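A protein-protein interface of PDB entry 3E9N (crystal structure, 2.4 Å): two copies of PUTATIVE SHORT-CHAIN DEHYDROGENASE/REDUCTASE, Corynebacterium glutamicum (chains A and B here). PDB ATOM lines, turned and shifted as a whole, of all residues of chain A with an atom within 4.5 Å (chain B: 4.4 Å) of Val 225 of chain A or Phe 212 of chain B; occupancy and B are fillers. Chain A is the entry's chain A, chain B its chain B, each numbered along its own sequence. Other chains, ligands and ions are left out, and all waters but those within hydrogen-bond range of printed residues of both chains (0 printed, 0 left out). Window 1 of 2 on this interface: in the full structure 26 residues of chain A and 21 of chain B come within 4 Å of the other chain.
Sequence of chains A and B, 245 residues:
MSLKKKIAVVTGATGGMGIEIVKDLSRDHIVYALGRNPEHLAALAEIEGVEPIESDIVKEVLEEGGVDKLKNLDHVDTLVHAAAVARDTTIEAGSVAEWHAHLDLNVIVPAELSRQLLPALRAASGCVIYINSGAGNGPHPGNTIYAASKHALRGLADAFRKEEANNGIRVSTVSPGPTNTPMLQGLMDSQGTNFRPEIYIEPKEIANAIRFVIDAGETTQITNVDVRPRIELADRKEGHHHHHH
Of the printed residues of chain B, Val 225 of chain A touches Phe 212 (3.8 Å), Ile 222 (3.9 Å) and Asn 224 (3.5 Å). Of chain A, only Asn 208 (3.8 Å), Ala 209 (3.7 Å), Phe 212 (3.7 Å) and Val 225 (3.8 Å) come within 4 Å of Phe 212 of chain B. Of the printed residues of chain A, Asn 224 of chain B touches Val 225 (3.5 Å) and Asp 226 (2.8 Å). Of the printed residues of chain B, Asn 208 of chain A touches Phe 212 (3.8 Å). Val 227 of chain A touches none of the printed residues of chain B. Ala 216 of chain B touches none of the printed residues of chain A. The nearest printed residue of chain B that does not touch Ala 209 of chain A is Ile 222 of chain B (5.6 Å).
N of Asp 226 of chain A is in hydrogen-bond range of O of Asn 224 of chain B, at 2.8 Å.
The backbone carbonyl oxygen of Val 225 of chain A lies within hydrogen-bond range of the backbone NH of Ser 175 of chain A (2.8 Å). The side-chain amide nitrogen of Asn 224 of chain A lies within hydrogen-bond range of the side-chain carboxylate of Asp 226 of chain A (2.8 Å). The backbone NH of Val 225 of chain A is in hydrogen-bond range of the backbone carbonyl oxygen of Thr 173 of chain A (3.0 Å). The side-chain hydroxyl (OG) of Ser 175 of chain A lies within hydrogen-bond range of the side-chain carboxylate (OD2) of Asp 226 of chain A (3.4 Å).
Asn 208 of chain A touches Phe 212 of chain B (O to CE1, 3.8 Å). CA of Ala 209 of chain A touches CZ of Phe 212 of chain B, 3.7 Å away. Asn 208 of chain B touches Phe 212 of chain A. Phe 212 of chain A touches Ala 209 of chain B (CZ to CA, 3.6 Å). Phe 212 of chain A touches Phe 212 of chain B (CD2 to CD2, 3.7 Å). Val 225 of chain A touches Phe 212 of chain B (CG1 to CE2, 3.8 Å). CG2 of Ile 222 of chain B touches CG1 of Val 225 of chain A (3.9 Å). CA of Val 225 of chain A touches O of Asn 224 of chain B, at 3.5 Å. Asp 226 of chain A touches Ile 222 of chain B.
Hydrophobic or aromatic side chains of chain A within 4 Å of the printed part of chain B: Ala 209, Phe 212 and Val 225. Along chain A the printed residues that touch a printed residue of chain B span positions 208 to 226. Of the 11 printed residues of chain B, 5 touch a printed residue of chain A. Among the printed residues, 10 pairs touch across the chains. Among the printed residues, no Asp or Glu carboxylate lies within 4 Å of a Lys or Arg side-chain nitrogen of the other chain.
Asn 208 of chain A touches Phe 212 of chain B, and with the chains exchanged Phe 212 of chain A touches Asn 208 of chain B. Ala 209 of chain A touches Phe 212 of chain B, and with the chains exchanged Phe 212 of chain A touches Ala 209 of chain B. Phe 212 of chain B touches its own counterpart, Phe 212 of chain A. Of the 10 pairs that touch across the chains among the printed residues, 5 have their exchanged pair printed and touching as well.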
ATOM      1  N   THR A 173      12.971  -5.012 -13.688  1.00  0.00           N
ATOM      2  CA  THR A 173      12.747  -3.956 -12.744  1.00  0.00           C
ATOM      3  C   THR A 173      11.724  -4.372 -11.743  1.00  0.00           C
ATOM      4  O   THR A 173      10.629  -4.765 -12.072  1.00  0.00           O
ATOM      5  CB  THR A 173      12.205  -2.692 -13.416  1.00  0.00           C
ATOM      6  OG1 THR A 173      11.026  -3.058 -14.145  1.00  0.00           O
ATOM      7  CG2 THR A 173      13.222  -2.136 -14.378  1.00  0.00           C
ATOM      8  N   VAL A 174      12.070  -4.270 -10.491  1.00  0.00           N
ATOM      9  CA  VAL A 174      11.129  -4.532  -9.482  1.00  0.00           C
ATOM     10  C   VAL A 174      10.756  -3.155  -8.989  1.00  0.00           C
ATOM     11  O   VAL A 174      11.639  -2.413  -8.574  1.00  0.00           O
ATOM     12  CB  VAL A 174      11.772  -5.410  -8.376  1.00  0.00           C
ATOM     13  CG1 VAL A 174      10.867  -5.472  -7.130  1.00  0.00           C
ATOM     14  CG2 VAL A 174      12.087  -6.811  -8.962  1.00  0.00           C
ATOM     15  N   SER A 175       9.468  -2.792  -9.049  1.00  0.00           N
ATOM     16  CA  SER A 175       9.084  -1.395  -8.726  1.00  0.00           C
ATOM     17  C   SER A 175       8.187  -1.273  -7.508  1.00  0.00           C
ATOM     18  O   SER A 175       6.962  -1.450  -7.592  1.00  0.00           O
ATOM     19  CB  SER A 175       8.408  -0.702  -9.901  1.00  0.00           C
ATOM     20  OG  SER A 175       8.900  -1.181 -11.142  1.00  0.00           O
ATOM     21  N   ASN A 208      11.805 -12.021  -2.341  1.00  0.00           N
ATOM     22  CA  ASN A 208      10.961 -12.960  -3.123  1.00  0.00           C
ATOM     23  C   ASN A 208      10.750 -12.528  -4.571  1.00  0.00           C
ATOM     24  O   ASN A 208      10.749 -13.376  -5.471  1.00  0.00           O
ATOM     25  CB  ASN A 208       9.603 -13.254  -2.440  1.00  0.00           C
ATOM     26  CG  ASN A 208       9.776 -13.702  -0.995  1.00  0.00           C
ATOM     27  OD1 ASN A 208      10.860 -14.078  -0.601  1.00  0.00           O
ATOM     28  ND2 ASN A 208       8.734 -13.585  -0.191  1.00  0.00           N
ATOM     29  N   ALA A 209      10.564 -11.219  -4.800  1.00  0.00           N
ATOM     30  CA  ALA A 209      10.363 -10.768  -6.166  1.00  0.00           C
ATOM     31  C   ALA A 209      11.598 -11.064  -6.974  1.00  0.00           C
ATOM     32  O   ALA A 209      11.495 -11.506  -8.123  1.00  0.00           O
ATOM     33  CB  ALA A 209      10.002  -9.266  -6.241  1.00  0.00           C
ATOM     34  N   PHE A 212      11.747 -14.782  -7.647  1.00  0.00           N
ATOM     35  CA  PHE A 212      10.846 -15.124  -8.726  1.00  0.00           C
ATOM     36  C   PHE A 212      11.444 -14.755 -10.091  1.00  0.00           C
ATOM     37  O   PHE A 212      11.229 -15.459 -11.087  1.00  0.00           O
ATOM     38  CB  PHE A 212       9.514 -14.413  -8.532  1.00  0.00           C
ATOM     39  CG  PHE A 212       8.584 -14.532  -9.709  1.00  0.00           C
ATOM     40  CD1 PHE A 212       8.006 -15.760 -10.022  1.00  0.00           C
ATOM     41  CD2 PHE A 212       8.269 -13.427 -10.468  1.00  0.00           C
ATOM     42  CE1 PHE A 212       7.161 -15.880 -11.091  1.00  0.00           C
ATOM     43  CE2 PHE A 212       7.382 -13.529 -11.530  1.00  0.00           C
ATOM     44  CZ  PHE A 212       6.837 -14.741 -11.848  1.00  0.00           C
ATOM     45  N   VAL A 213      12.196 -13.653 -10.158  1.00  0.00           N
ATOM     46  CA  VAL A 213      12.622 -13.182 -11.473  1.00  0.00           C
ATOM     47  C   VAL A 213      13.726 -14.066 -12.049  1.00  0.00           C
ATOM     48  O   VAL A 213      13.715 -14.457 -13.247  1.00  0.00           O
ATOM     49  CB  VAL A 213      13.083 -11.696 -11.425  1.00  0.00           C
ATOM     50  CG1 VAL A 213      14.081 -11.378 -12.567  1.00  0.00           C
ATOM     51  CG2 VAL A 213      11.857 -10.718 -11.435  1.00  0.00           C
ATOM     52  N   ILE A 222      10.891 -12.060 -16.901  1.00  0.00           N
ATOM     53  CA  ILE A 222       9.962 -11.297 -16.088  1.00  0.00           C
ATOM     54  C   ILE A 222      10.614  -9.951 -16.075  1.00  0.00           C
ATOM     55  O   ILE A 222      11.594  -9.714 -15.306  1.00  0.00           O
ATOM     56  CB  ILE A 222       9.870 -11.860 -14.671  1.00  0.00           C
ATOM     57  CG1 ILE A 222       9.656 -13.384 -14.738  1.00  0.00           C
ATOM     58  CG2 ILE A 222       8.809 -11.070 -13.785  1.00  0.00           C
ATOM     59  CD1 ILE A 222       8.223 -13.781 -15.130  1.00  0.00           C
ATOM     60  N   ASN A 224       9.113  -6.834 -15.486  1.00  0.00           N
ATOM     61  CA  ASN A 224       8.729  -5.885 -14.469  1.00  0.00           C
ATOM     62  C   ASN A 224       7.774  -6.484 -13.436  1.00  0.00           C
ATOM     63  O   ASN A 224       6.973  -7.363 -13.748  1.00  0.00           O
ATOM     64  CB  ASN A 224       8.254  -4.539 -15.071  1.00  0.00           C
ATOM     65  CG  ASN A 224       7.864  -3.512 -13.988  1.00  0.00           C
ATOM     66  OD1 ASN A 224       8.723  -2.787 -13.339  1.00  0.00           O
ATOM     67  ND2 ASN A 224       6.536  -3.424 -13.771  1.00  0.00           N
ATOM     68  N   VAL A 225       7.937  -6.070 -12.194  1.00  0.00           N
ATOM     69  CA  VAL A 225       7.074  -6.549 -11.092  1.00  0.00           C
ATOM     70  C   VAL A 225       6.685  -5.317 -10.315  1.00  0.00           C
ATOM     71  O   VAL A 225       7.544  -4.632  -9.805  1.00  0.00           O
ATOM     72  CB  VAL A 225       7.792  -7.535 -10.138  1.00  0.00           C
ATOM     73  CG1 VAL A 225       6.891  -7.954  -9.023  1.00  0.00           C
ATOM     74  CG2 VAL A 225       8.340  -8.794 -10.888  1.00  0.00           C
ATOM     75  N   ASP A 226       5.403  -4.964 -10.283  1.00  0.00           N
ATOM     76  CA  ASP A 226       4.963  -3.785  -9.541  1.00  0.00           C
ATOM     77  C   ASP A 226       4.492  -4.228  -8.135  1.00  0.00           C
ATOM     78  O   ASP A 226       3.685  -5.122  -7.988  1.00  0.00           O
ATOM     79  CB  ASP A 226       3.934  -3.001 -10.364  1.00  0.00           C
ATOM     80  CG  ASP A 226       4.538  -2.463 -11.692  1.00  0.00           C
ATOM     81  OD1 ASP A 226       3.976  -2.758 -12.806  1.00  0.00           O
ATOM     82  OD2 ASP A 226       5.624  -1.777 -11.660  1.00  0.00           O
ATOM     83  N   VAL A 227       5.081  -3.633  -7.105  1.00  0.00           N
ATOM     84  CA  VAL A 227       4.909  -4.063  -5.721  1.00  0.00           C
ATOM     85  C   VAL A 227       4.315  -2.906  -4.900  1.00  0.00           C
ATOM     86  O   VAL A 227       4.745  -1.789  -5.030  1.00  0.00           O
ATOM     87  CB  VAL A 227       6.293  -4.511  -5.101  1.00  0.00           C
ATOM     88  CG1 VAL A 227       6.138  -4.912  -3.658  1.00  0.00           C
ATOM     89  CG2 VAL A 227       6.903  -5.632  -5.911  1.00  0.00           C
ATOM     90  N   ASN B 208       3.180 -19.946 -12.532  1.00  0.00           N
ATOM     91  CA  ASN B 208       4.173 -19.462 -11.590  1.00  0.00           C
ATOM     92  C   ASN B 208       3.934 -18.015 -11.236  1.00  0.00           C
ATOM     93  O   ASN B 208       4.114 -17.645 -10.082  1.00  0.00           O
ATOM     94  CB  ASN B 208       5.586 -19.581 -12.161  1.00  0.00           C
ATOM     95  CG  ASN B 208       6.038 -20.997 -12.262  1.00  0.00           C
ATOM     96  OD1 ASN B 208       5.413 -21.905 -11.705  1.00  0.00           O
ATOM     97  ND2 ASN B 208       7.144 -21.211 -12.984  1.00  0.00           N
ATOM     98  N   ALA B 209       3.597 -17.190 -12.227  1.00  0.00           N
ATOM     99  CA  ALA B 209       3.408 -15.806 -11.931  1.00  0.00           C
ATOM    100  C   ALA B 209       2.190 -15.632 -11.040  1.00  0.00           C
ATOM    101  O   ALA B 209       2.167 -14.761 -10.147  1.00  0.00           O
ATOM    102  CB  ALA B 209       3.266 -14.972 -13.207  1.00  0.00           C
ATOM    103  N   ILE B 210       1.184 -16.478 -11.250  1.00  0.00           N
ATOM    104  CA  ILE B 210       0.000 -16.343 -10.450  1.00  0.00           C
ATOM    105  C   ILE B 210       0.298 -16.780  -9.036  1.00  0.00           C
ATOM    106  O   ILE B 210      -0.154 -16.145  -8.058  1.00  0.00           O
ATOM    107  CB  ILE B 210      -1.221 -16.993 -11.103  1.00  0.00           C
ATOM    108  CG1 ILE B 210      -1.724 -16.025 -12.192  1.00  0.00           C
ATOM    109  CG2 ILE B 210      -2.309 -17.242 -10.062  1.00  0.00           C
ATOM    110  CD1 ILE B 210      -2.317 -16.622 -13.327  1.00  0.00           C
ATOM    111  N   ARG B 211       1.108 -17.815  -8.914  1.00  0.00           N
ATOM    112  CA  ARG B 211       1.434 -18.366  -7.624  1.00  0.00           C
ATOM    113  C   ARG B 211       2.261 -17.312  -6.860  1.00  0.00           C
ATOM    114  O   ARG B 211       2.097 -17.134  -5.657  1.00  0.00           O
ATOM    115  CB  ARG B 211       2.193 -19.682  -7.809  1.00  0.00           C
ATOM    116  CG  ARG B 211       2.961 -20.173  -6.573  1.00  0.00           C
ATOM    117  CD  ARG B 211       2.047 -20.281  -5.303  1.00  0.00           C
ATOM    118  NE  ARG B 211       0.866 -21.146  -5.487  1.00  0.00           N
ATOM    119  CZ  ARG B 211      -0.026 -21.386  -4.524  1.00  0.00           C
ATOM    120  NH1 ARG B 211      -1.053 -22.195  -4.746  1.00  0.00           N
ATOM    121  NH2 ARG B 211       0.109 -20.798  -3.325  1.00  0.00           N
ATOM    122  N   PHE B 212       3.152 -16.614  -7.560  1.00  0.00           N
ATOM    123  CA  PHE B 212       3.924 -15.558  -6.932  1.00  0.00           C
ATOM    124  C   PHE B 212       2.994 -14.392  -6.481  1.00  0.00           C
ATOM    125  O   PHE B 212       3.138 -13.840  -5.378  1.00  0.00           O
ATOM    126  CB  PHE B 212       5.013 -15.079  -7.896  1.00  0.00           C
ATOM    127  CG  PHE B 212       5.638 -13.796  -7.498  1.00  0.00           C
ATOM    128  CD1 PHE B 212       6.447 -13.738  -6.379  1.00  0.00           C
ATOM    129  CD2 PHE B 212       5.430 -12.647  -8.243  1.00  0.00           C
ATOM    130  CE1 PHE B 212       7.039 -12.534  -6.010  1.00  0.00           C
ATOM    131  CE2 PHE B 212       5.959 -11.445  -7.859  1.00  0.00           C
ATOM    132  CZ  PHE B 212       6.777 -11.370  -6.751  1.00  0.00           C
ATOM    133  N   VAL B 213       2.017 -14.037  -7.305  1.00  0.00           N
ATOM    134  CA  VAL B 213       1.096 -12.980  -6.913  1.00  0.00           C
ATOM    135  C   VAL B 213       0.333 -13.318  -5.634  1.00  0.00           C
ATOM    136  O   VAL B 213       0.313 -12.538  -4.680  1.00  0.00           O
ATOM    137  CB  VAL B 213       0.126 -12.583  -8.047  1.00  0.00           C
ATOM    138  CG1 VAL B 213      -0.995 -11.684  -7.491  1.00  0.00           C
ATOM    139  CG2 VAL B 213       0.915 -11.872  -9.172  1.00  0.00           C
ATOM    140  N   ILE B 214      -0.279 -14.478  -5.578  1.00  0.00           N
ATOM    141  CA  ILE B 214      -1.088 -14.742  -4.416  1.00  0.00           C
ATOM    142  C   ILE B 214      -0.270 -15.168  -3.186  1.00  0.00           C
ATOM    143  O   ILE B 214      -0.852 -15.280  -2.098  1.00  0.00           O
ATOM    144  CB  ILE B 214      -2.177 -15.776  -4.711  1.00  0.00           C
ATOM    145  CG1 ILE B 214      -1.523 -17.182  -4.827  1.00  0.00           C
ATOM    146  CG2 ILE B 214      -3.008 -15.300  -5.907  1.00  0.00           C
ATOM    147  CD1 ILE B 214      -2.459 -18.364  -4.943  1.00  0.00           C
ATOM    148  N   ASP B 215       1.056 -15.385  -3.319  1.00  0.00           N
ATOM    149  CA  ASP B 215       1.852 -15.837  -2.152  1.00  0.00           C
ATOM    150  C   ASP B 215       2.391 -14.643  -1.367  1.00  0.00           C
ATOM    151  O   ASP B 215       2.997 -14.809  -0.316  1.00  0.00           O
ATOM    152  CB  ASP B 215       3.013 -16.752  -2.546  1.00  0.00           C
ATOM    153  CG  ASP B 215       2.673 -18.254  -2.453  1.00  0.00           C
ATOM    154  OD1 ASP B 215       1.525 -18.599  -2.084  1.00  0.00           O
ATOM    155  OD2 ASP B 215       3.578 -19.105  -2.784  1.00  0.00           O
ATOM    156  N   ALA B 216       2.165 -13.449  -1.898  1.00  0.00           N
ATOM    157  CA  ALA B 216       2.565 -12.206  -1.254  1.00  0.00           C
ATOM    158  C   ALA B 216       2.166 -12.160   0.236  1.00  0.00           C
ATOM    159  O   ALA B 216       1.083 -12.591   0.608  1.00  0.00           O
ATOM    160  CB  ALA B 216       1.972 -11.003  -2.016  1.00  0.00           C
ATOM    161  N   ILE B 222       1.201  -7.715  -5.143  1.00  0.00           N
ATOM    162  CA  ILE B 222       1.870  -7.608  -6.415  1.00  0.00           C
ATOM    163  C   ILE B 222       0.801  -7.209  -7.414  1.00  0.00           C
ATOM    164  O   ILE B 222      -0.038  -8.032  -7.747  1.00  0.00           O
ATOM    165  CB  ILE B 222       2.419  -8.971  -6.836  1.00  0.00           C
ATOM    166  CG1 ILE B 222       3.219  -9.625  -5.700  1.00  0.00           C
ATOM    167  CG2 ILE B 222       3.231  -8.834  -8.087  1.00  0.00           C
ATOM    168  CD1 ILE B 222       4.484  -8.804  -5.253  1.00  0.00           C
ATOM    169  N   ASN B 224       1.120  -5.918 -10.686  1.00  0.00           N
ATOM    170  CA  ASN B 224       1.329  -6.298 -12.055  1.00  0.00           C
ATOM    171  C   ASN B 224       2.656  -7.057 -12.214  1.00  0.00           C
ATOM    172  O   ASN B 224       3.602  -6.810 -11.457  1.00  0.00           O
ATOM    173  CB  ASN B 224       1.263  -5.076 -12.976  1.00  0.00           C
ATOM    174  CG  ASN B 224       1.507  -5.440 -14.448  1.00  0.00           C
ATOM    175  OD1 ASN B 224       0.688  -6.119 -15.109  1.00  0.00           O
ATOM    176  ND2 ASN B 224       2.663  -5.026 -14.959  1.00  0.00           N
